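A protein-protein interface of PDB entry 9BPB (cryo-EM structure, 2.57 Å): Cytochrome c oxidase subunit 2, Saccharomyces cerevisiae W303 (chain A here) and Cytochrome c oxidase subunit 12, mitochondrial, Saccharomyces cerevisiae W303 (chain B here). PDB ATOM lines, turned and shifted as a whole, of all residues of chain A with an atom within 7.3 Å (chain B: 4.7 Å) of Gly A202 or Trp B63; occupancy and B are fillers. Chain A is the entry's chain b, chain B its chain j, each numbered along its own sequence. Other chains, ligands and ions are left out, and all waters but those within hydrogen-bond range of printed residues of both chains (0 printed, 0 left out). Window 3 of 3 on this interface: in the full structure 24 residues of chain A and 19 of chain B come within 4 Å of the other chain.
OG1 of Thr A180 is in hydrogen-bond range of O of Arg A203 (3.0 Å). OG1 of Thr A180 sits at hydrogen-bond distance from O of Thr A200 (3.3 Å).
Among the printed residues, merely in contact across the chains: Thr A180 with Pro B60 (3.9 Å), Gly A202 with Trp B63 (3.4 Å), Arg A203 with Thr B24 (3.6 Å), Leu A204 with Thr B24 (3.5 Å) and Leu A204 with Pro B60 (3.8 Å).
Of the printed residues of chain B, Thr A180 touches Pro B60 (3.9 Å). Printed residues of chain B within 4 Å of Gly A202: Trp B63 (3.4 Å). Printed residues of chain B within 4 Å of Arg A203: Thr B24 (3.6 Å). Printed residues of chain B within 4 Å of Leu A204: Thr B24 and Pro B60. Of the printed residues of chain A, Thr B24 touches Arg A203 and Leu A204. Of the printed residues of chain A, Pro B60 touches Thr A180 and Leu A204. Trp B63 touches one residue of chain A. The nearest residue of chain A that does not touch Trp B63 is Leu A204 (4.1 Å).
Hydrophobic or aromatic side chains of chain A within 4 Å of the printed part of chain B: Leu A204. Among the printed residues, 5 pairs touch across the chains.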
ATOM      1  N   ILE A 120     -23.602  -6.463   1.608  1.00  0.00           N
ATOM      2  CA  ILE A 120     -22.256  -6.631   0.992  1.00  0.00           C
ATOM      3  C   ILE A 120     -22.115  -8.103   0.614  1.00  0.00           C
ATOM      4  O   ILE A 120     -22.344  -8.958   1.488  1.00  0.00           O
ATOM      5  CB  ILE A 120     -21.146  -6.200   1.972  1.00  0.00           C
ATOM      6  CG1 ILE A 120     -21.383  -4.798   2.541  1.00  0.00           C
ATOM      7  CG2 ILE A 120     -19.776  -6.323   1.321  1.00  0.00           C
ATOM      8  CD1 ILE A 120     -22.249  -4.766   3.777  1.00  0.00           C
ATOM      9  N   VAL A 179     -25.499  -0.972  -1.001  1.00  0.00           N
ATOM     10  CA  VAL A 179     -24.881  -2.233  -1.389  1.00  0.00           C
ATOM     11  C   VAL A 179     -23.474  -1.978  -1.907  1.00  0.00           C
ATOM     12  O   VAL A 179     -23.170  -0.913  -2.455  1.00  0.00           O
ATOM     13  CB  VAL A 179     -25.709  -2.979  -2.455  1.00  0.00           C
ATOM     14  CG1 VAL A 179     -27.099  -3.295  -1.929  1.00  0.00           C
ATOM     15  CG2 VAL A 179     -25.762  -2.175  -3.734  1.00  0.00           C
ATOM     16  N   THR A 180     -22.614  -2.976  -1.726  1.00  0.00           N
ATOM     17  CA  THR A 180     -21.267  -2.956  -2.275  1.00  0.00           C
ATOM     18  C   THR A 180     -20.826  -4.391  -2.519  1.00  0.00           C
ATOM     19  O   THR A 180     -21.635  -5.323  -2.506  1.00  0.00           O
ATOM     20  CB  THR A 180     -20.297  -2.216  -1.350  1.00  0.00           C
ATOM     21  OG1 THR A 180     -18.996  -2.176  -1.950  1.00  0.00           O
ATOM     22  CG2 THR A 180     -20.210  -2.899  -0.001  1.00  0.00           C
ATOM     23  N   ALA A 181     -19.528  -4.567  -2.749  1.00  0.00           N
ATOM     24  CA  ALA A 181     -18.955  -5.883  -2.974  1.00  0.00           C
ATOM     25  C   ALA A 181     -17.522  -5.896  -2.471  1.00  0.00           C
ATOM     26  O   ALA A 181     -16.913  -4.850  -2.236  1.00  0.00           O
ATOM     27  CB  ALA A 181     -19.006  -6.275  -4.453  1.00  0.00           C
ATOM     28  N   ALA A 182     -16.986  -7.103  -2.295  1.00  0.00           N
ATOM     29  CA  ALA A 182     -15.628  -7.280  -1.793  1.00  0.00           C
ATOM     30  C   ALA A 182     -14.711  -7.916  -2.834  1.00  0.00           C
ATOM     31  O   ALA A 182     -13.591  -7.444  -3.051  1.00  0.00           O
ATOM     32  CB  ALA A 182     -15.650  -8.119  -0.510  1.00  0.00           C
ATOM     33  N   ALA A 199     -23.912  -3.126  -7.330  1.00  0.00           N
ATOM     34  CA  ALA A 199     -23.048  -3.575  -6.209  1.00  0.00           C
ATOM     35  C   ALA A 199     -21.604  -3.777  -6.684  1.00  0.00           C
ATOM     36  O   ALA A 199     -21.146  -4.925  -6.664  1.00  0.00           O
ATOM     37  CB  ALA A 199     -23.608  -4.790  -5.535  1.00  0.00           C
ATOM     38  N   THR A 200     -20.925  -2.692  -7.074  1.00  0.00           N
ATOM     39  CA  THR A 200     -19.498  -2.679  -7.519  1.00  0.00           C
ATOM     40  C   THR A 200     -18.555  -2.780  -6.311  1.00  0.00           C
ATOM     41  O   THR A 200     -18.883  -2.231  -5.249  1.00  0.00           O
ATOM     42  CB  THR A 200     -19.236  -1.469  -8.423  1.00  0.00           C
ATOM     43  OG1 THR A 200     -19.931  -1.694  -9.648  1.00  0.00           O
ATOM     44  CG2 THR A 200     -17.773  -1.221  -8.715  1.00  0.00           C
ATOM     45  N   PRO A 201     -17.404  -3.465  -6.432  1.00  0.00           N
ATOM     46  CA  PRO A 201     -16.496  -3.759  -5.308  1.00  0.00           C
ATOM     47  C   PRO A 201     -15.878  -2.546  -4.628  1.00  0.00           C
ATOM     48  O   PRO A 201     -15.112  -2.734  -3.675  1.00  0.00           O
ATOM     49  CB  PRO A 201     -15.407  -4.623  -5.955  1.00  0.00           C
ATOM     50  CG  PRO A 201     -16.082  -5.276  -7.090  1.00  0.00           C
ATOM     51  CD  PRO A 201     -17.080  -4.285  -7.613  1.00  0.00           C
ATOM     52  N   GLY A 202     -16.161  -1.326  -5.071  1.00  0.00           N
ATOM     53  CA  GLY A 202     -15.577  -0.170  -4.421  1.00  0.00           C
ATOM     54  C   GLY A 202     -16.544   0.969  -4.166  1.00  0.00           C
ATOM     55  O   GLY A 202     -16.175   1.974  -3.555  1.00  0.00           O
ATOM     56  N   ARG A 203     -17.784   0.820  -4.622  1.00  0.00           N
ATOM     57  CA  ARG A 203     -18.776   1.881  -4.567  1.00  0.00           C
ATOM     58  C   ARG A 203     -19.906   1.513  -3.615  1.00  0.00           C
ATOM     59  O   ARG A 203     -20.045   0.362  -3.198  1.00  0.00           O
ATOM     60  CB  ARG A 203     -19.338   2.173  -5.962  1.00  0.00           C
ATOM     61  CG  ARG A 203     -18.392   2.958  -6.844  1.00  0.00           C
ATOM     62  CD  ARG A 203     -19.028   3.306  -8.176  1.00  0.00           C
ATOM     63  NE  ARG A 203     -20.235   4.108  -8.021  1.00  0.00           N
ATOM     64  CZ  ARG A 203     -20.911   4.645  -9.028  1.00  0.00           C
ATOM     65  NH1 ARG A 203     -20.502   4.520 -10.280  1.00  0.00           N
ATOM     66  NH2 ARG A 203     -22.022   5.328  -8.773  1.00  0.00           N
ATOM     67  N   LEU A 204     -20.716   2.516  -3.273  1.00  0.00           N
ATOM     68  CA  LEU A 204     -21.887   2.343  -2.418  1.00  0.00           C
ATOM     69  C   LEU A 204     -23.081   3.015  -3.084  1.00  0.00           C
ATOM     70  O   LEU A 204     -23.285   4.223  -2.925  1.00  0.00           O
ATOM     71  CB  LEU A 204     -21.642   2.924  -1.026  1.00  0.00           C
ATOM     72  CG  LEU A 204     -20.444   2.402  -0.238  1.00  0.00           C
ATOM     73  CD1 LEU A 204     -20.124   3.330   0.918  1.00  0.00           C
ATOM     74  CD2 LEU A 204     -20.723   1.002   0.269  1.00  0.00           C
ATOM     75  N   THR B  24     -20.172   7.021  -1.963  1.00  0.00           N
ATOM     76  CA  THR B  24     -18.844   6.726  -1.430  1.00  0.00           C
ATOM     77  C   THR B  24     -18.251   7.927  -0.705  1.00  0.00           C
ATOM     78  O   THR B  24     -17.656   7.777   0.369  1.00  0.00           O
ATOM     79  CB  THR B  24     -17.910   6.275  -2.553  1.00  0.00           C
ATOM     80  OG1 THR B  24     -17.529   7.406  -3.345  1.00  0.00           O
ATOM     81  CG2 THR B  24     -18.598   5.261  -3.435  1.00  0.00           C
ATOM     82  N   PRO B  60     -19.462   0.094   5.115  1.00  0.00           N
ATOM     83  CA  PRO B  60     -19.156  -1.305   5.433  1.00  0.00           C
ATOM     84  C   PRO B  60     -18.161  -1.402   6.579  1.00  0.00           C
ATOM     85  O   PRO B  60     -17.319  -0.523   6.775  1.00  0.00           O
ATOM     86  CB  PRO B  60     -18.562  -1.847   4.127  1.00  0.00           C
ATOM     87  CG  PRO B  60     -19.022  -0.894   3.070  1.00  0.00           C
ATOM     88  CD  PRO B  60     -19.085   0.441   3.737  1.00  0.00           C
ATOM     89  N   LEU B  61     -18.277  -2.484   7.350  1.00  0.00           N
ATOM     90  CA  LEU B  61     -17.440  -2.626   8.536  1.00  0.00           C
ATOM     91  C   LEU B  61     -15.966  -2.732   8.174  1.00  0.00           C
ATOM     92  O   LEU B  61     -15.145  -1.976   8.700  1.00  0.00           O
ATOM     93  CB  LEU B  61     -17.874  -3.839   9.356  1.00  0.00           C
ATOM     94  CG  LEU B  61     -19.142  -3.688  10.200  1.00  0.00           C
ATOM     95  CD1 LEU B  61     -19.385  -4.939  11.029  1.00  0.00           C
ATOM     96  CD2 LEU B  61     -19.055  -2.462  11.093  1.00  0.00           C
ATOM     97  N   ASP B  62     -15.614  -3.632   7.252  1.00  0.00           N
ATOM     98  CA  ASP B  62     -14.207  -3.922   6.994  1.00  0.00           C
ATOM     99  C   ASP B  62     -13.441  -2.713   6.471  1.00  0.00           C
ATOM    100  O   ASP B  62     -12.213  -2.675   6.600  1.00  0.00           O
ATOM    101  CB  ASP B  62     -14.073  -5.089   6.012  1.00  0.00           C
ATOM    102  CG  ASP B  62     -14.763  -4.827   4.692  1.00  0.00           C
ATOM    103  OD1 ASP B  62     -14.114  -4.266   3.786  1.00  0.00           O
ATOM    104  OD2 ASP B  62     -15.949  -5.193   4.558  1.00  0.00           O
ATOM    105  N   TRP B  63     -14.130  -1.730   5.888  1.00  0.00           N
ATOM    106  CA  TRP B  63     -13.459  -0.495   5.498  1.00  0.00           C
ATOM    107  C   TRP B  63     -12.913   0.240   6.714  1.00  0.00           C
ATOM    108  O   TRP B  63     -11.846   0.858   6.649  1.00  0.00           O
ATOM    109  CB  TRP B  63     -14.419   0.407   4.724  1.00  0.00           C
ATOM    110  CG  TRP B  63     -14.747  -0.078   3.353  1.00  0.00           C
ATOM    111  CD1 TRP B  63     -14.606  -1.345   2.875  1.00  0.00           C
ATOM    112  CD2 TRP B  63     -15.288   0.698   2.278  1.00  0.00           C
ATOM    113  NE1 TRP B  63     -15.020  -1.408   1.568  1.00  0.00           N
ATOM    114  CE2 TRP B  63     -15.444  -0.165   1.178  1.00  0.00           C
ATOM    115  CE3 TRP B  63     -15.653   2.041   2.140  1.00  0.00           C
ATOM    116  CZ2 TRP B  63     -15.949   0.269  -0.045  1.00  0.00           C
ATOM    117  CZ3 TRP B  63     -16.153   2.470   0.924  1.00  0.00           C
ATOM    118  CH2 TRP B  63     -16.297   1.587  -0.151  1.00  0.00           C
ATOM    119  N   ILE B  64     -13.642   0.192   7.832  1.00  0.00           N
ATOM    120  CA  ILE B  64     -13.217   0.902   9.034  1.00  0.00           C
ATOM    121  C   ILE B  64     -11.910   0.331   9.572  1.00  0.00           C
ATOM    122  O   ILE B  64     -10.991   1.081   9.924  1.00  0.00           O
ATOM    123  CB  ILE B  64     -14.333   0.874  10.096  1.00  0.00           C
ATOM    124  CG1 ILE B  64     -15.684   1.214   9.463  1.00  0.00           C
ATOM    125  CG2 ILE B  64     -14.019   1.839  11.224  1.00  0.00           C
ATOM    126  CD1 ILE B  64     -15.747   2.601   8.860  1.00  0.00           C
ATOM    127  N   GLU B  65     -11.797  -1.000   9.647  1.00  0.00           N
ATOM    128  CA  GLU B  65     -10.558  -1.593  10.144  1.00  0.00           C
ATOM    129  C   GLU B  65      -9.396  -1.340   9.191  1.00  0.00           C
ATOM    130  O   GLU B  65      -8.256  -1.158   9.633  1.00  0.00           O
ATOM    131  CB  GLU B  65     -10.718  -3.094  10.396  1.00  0.00           C
ATOM    132  CG  GLU B  65     -11.609  -3.460  11.578  1.00  0.00           C
ATOM    133  CD  GLU B  65     -13.072  -3.506  11.223  1.00  0.00           C
ATOM    134  OE1 GLU B  65     -13.389  -3.342  10.033  1.00  0.00           O
ATOM    135  OE2 GLU B  65     -13.903  -3.705  12.132  1.00  0.00           O
ATOM    136  N   LYS B  66      -9.657  -1.339   7.882  1.00  0.00           N
ATOM    137  CA  LYS B  66      -8.592  -1.012   6.939  1.00  0.00           C
ATOM    138  C   LYS B  66      -8.113   0.421   7.130  1.00  0.00           C
ATOM    139  O   LYS B  66      -6.905   0.683   7.127  1.00  0.00           O
ATOM    140  CB  LYS B  66      -9.061  -1.224   5.503  1.00  0.00           C
ATOM    141  CG  LYS B  66      -7.965  -0.986   4.481  1.00  0.00           C
ATOM    142  CD  LYS B  66      -8.459  -1.206   3.069  1.00  0.00           C
ATOM    143  CE  LYS B  66      -9.298  -0.032   2.602  1.00  0.00           C
ATOM    144  NZ  LYS B  66      -9.629  -0.131   1.155  1.00  0.00           N
ATOM    145  N   TRP B  67      -9.044   1.362   7.306  1.00  0.00           N
ATOM    146  CA  TRP B  67      -8.654   2.750   7.518  1.00  0.00           C
ATOM    147  C   TRP B  67      -8.052   2.955   8.900  1.00  0.00           C
ATOM    148  O   TRP B  67      -7.316   3.925   9.114  1.00  0.00           O
ATOM    149  CB  TRP B  67      -9.856   3.670   7.319  1.00  0.00           C
ATOM    150  CG  TRP B  67     -10.264   3.814   5.886  1.00  0.00           C
ATOM    151  CD1 TRP B  67      -9.472   3.645   4.789  1.00  0.00           C
ATOM    152  CD2 TRP B  67     -11.567   4.144   5.393  1.00  0.00           C
ATOM    153  NE1 TRP B  67     -10.199   3.852   3.644  1.00  0.00           N
ATOM    154  CE2 TRP B  67     -11.489   4.158   3.986  1.00  0.00           C
ATOM    155  CE3 TRP B  67     -12.792   4.427   6.003  1.00  0.00           C
ATOM    156  CZ2 TRP B  67     -12.588   4.447   3.183  1.00  0.00           C
ATOM    157  CZ3 TRP B  67     -13.881   4.714   5.201  1.00  0.00           C
ATOM    158  CH2 TRP B  67     -13.772   4.721   3.808  1.00  0.00           C
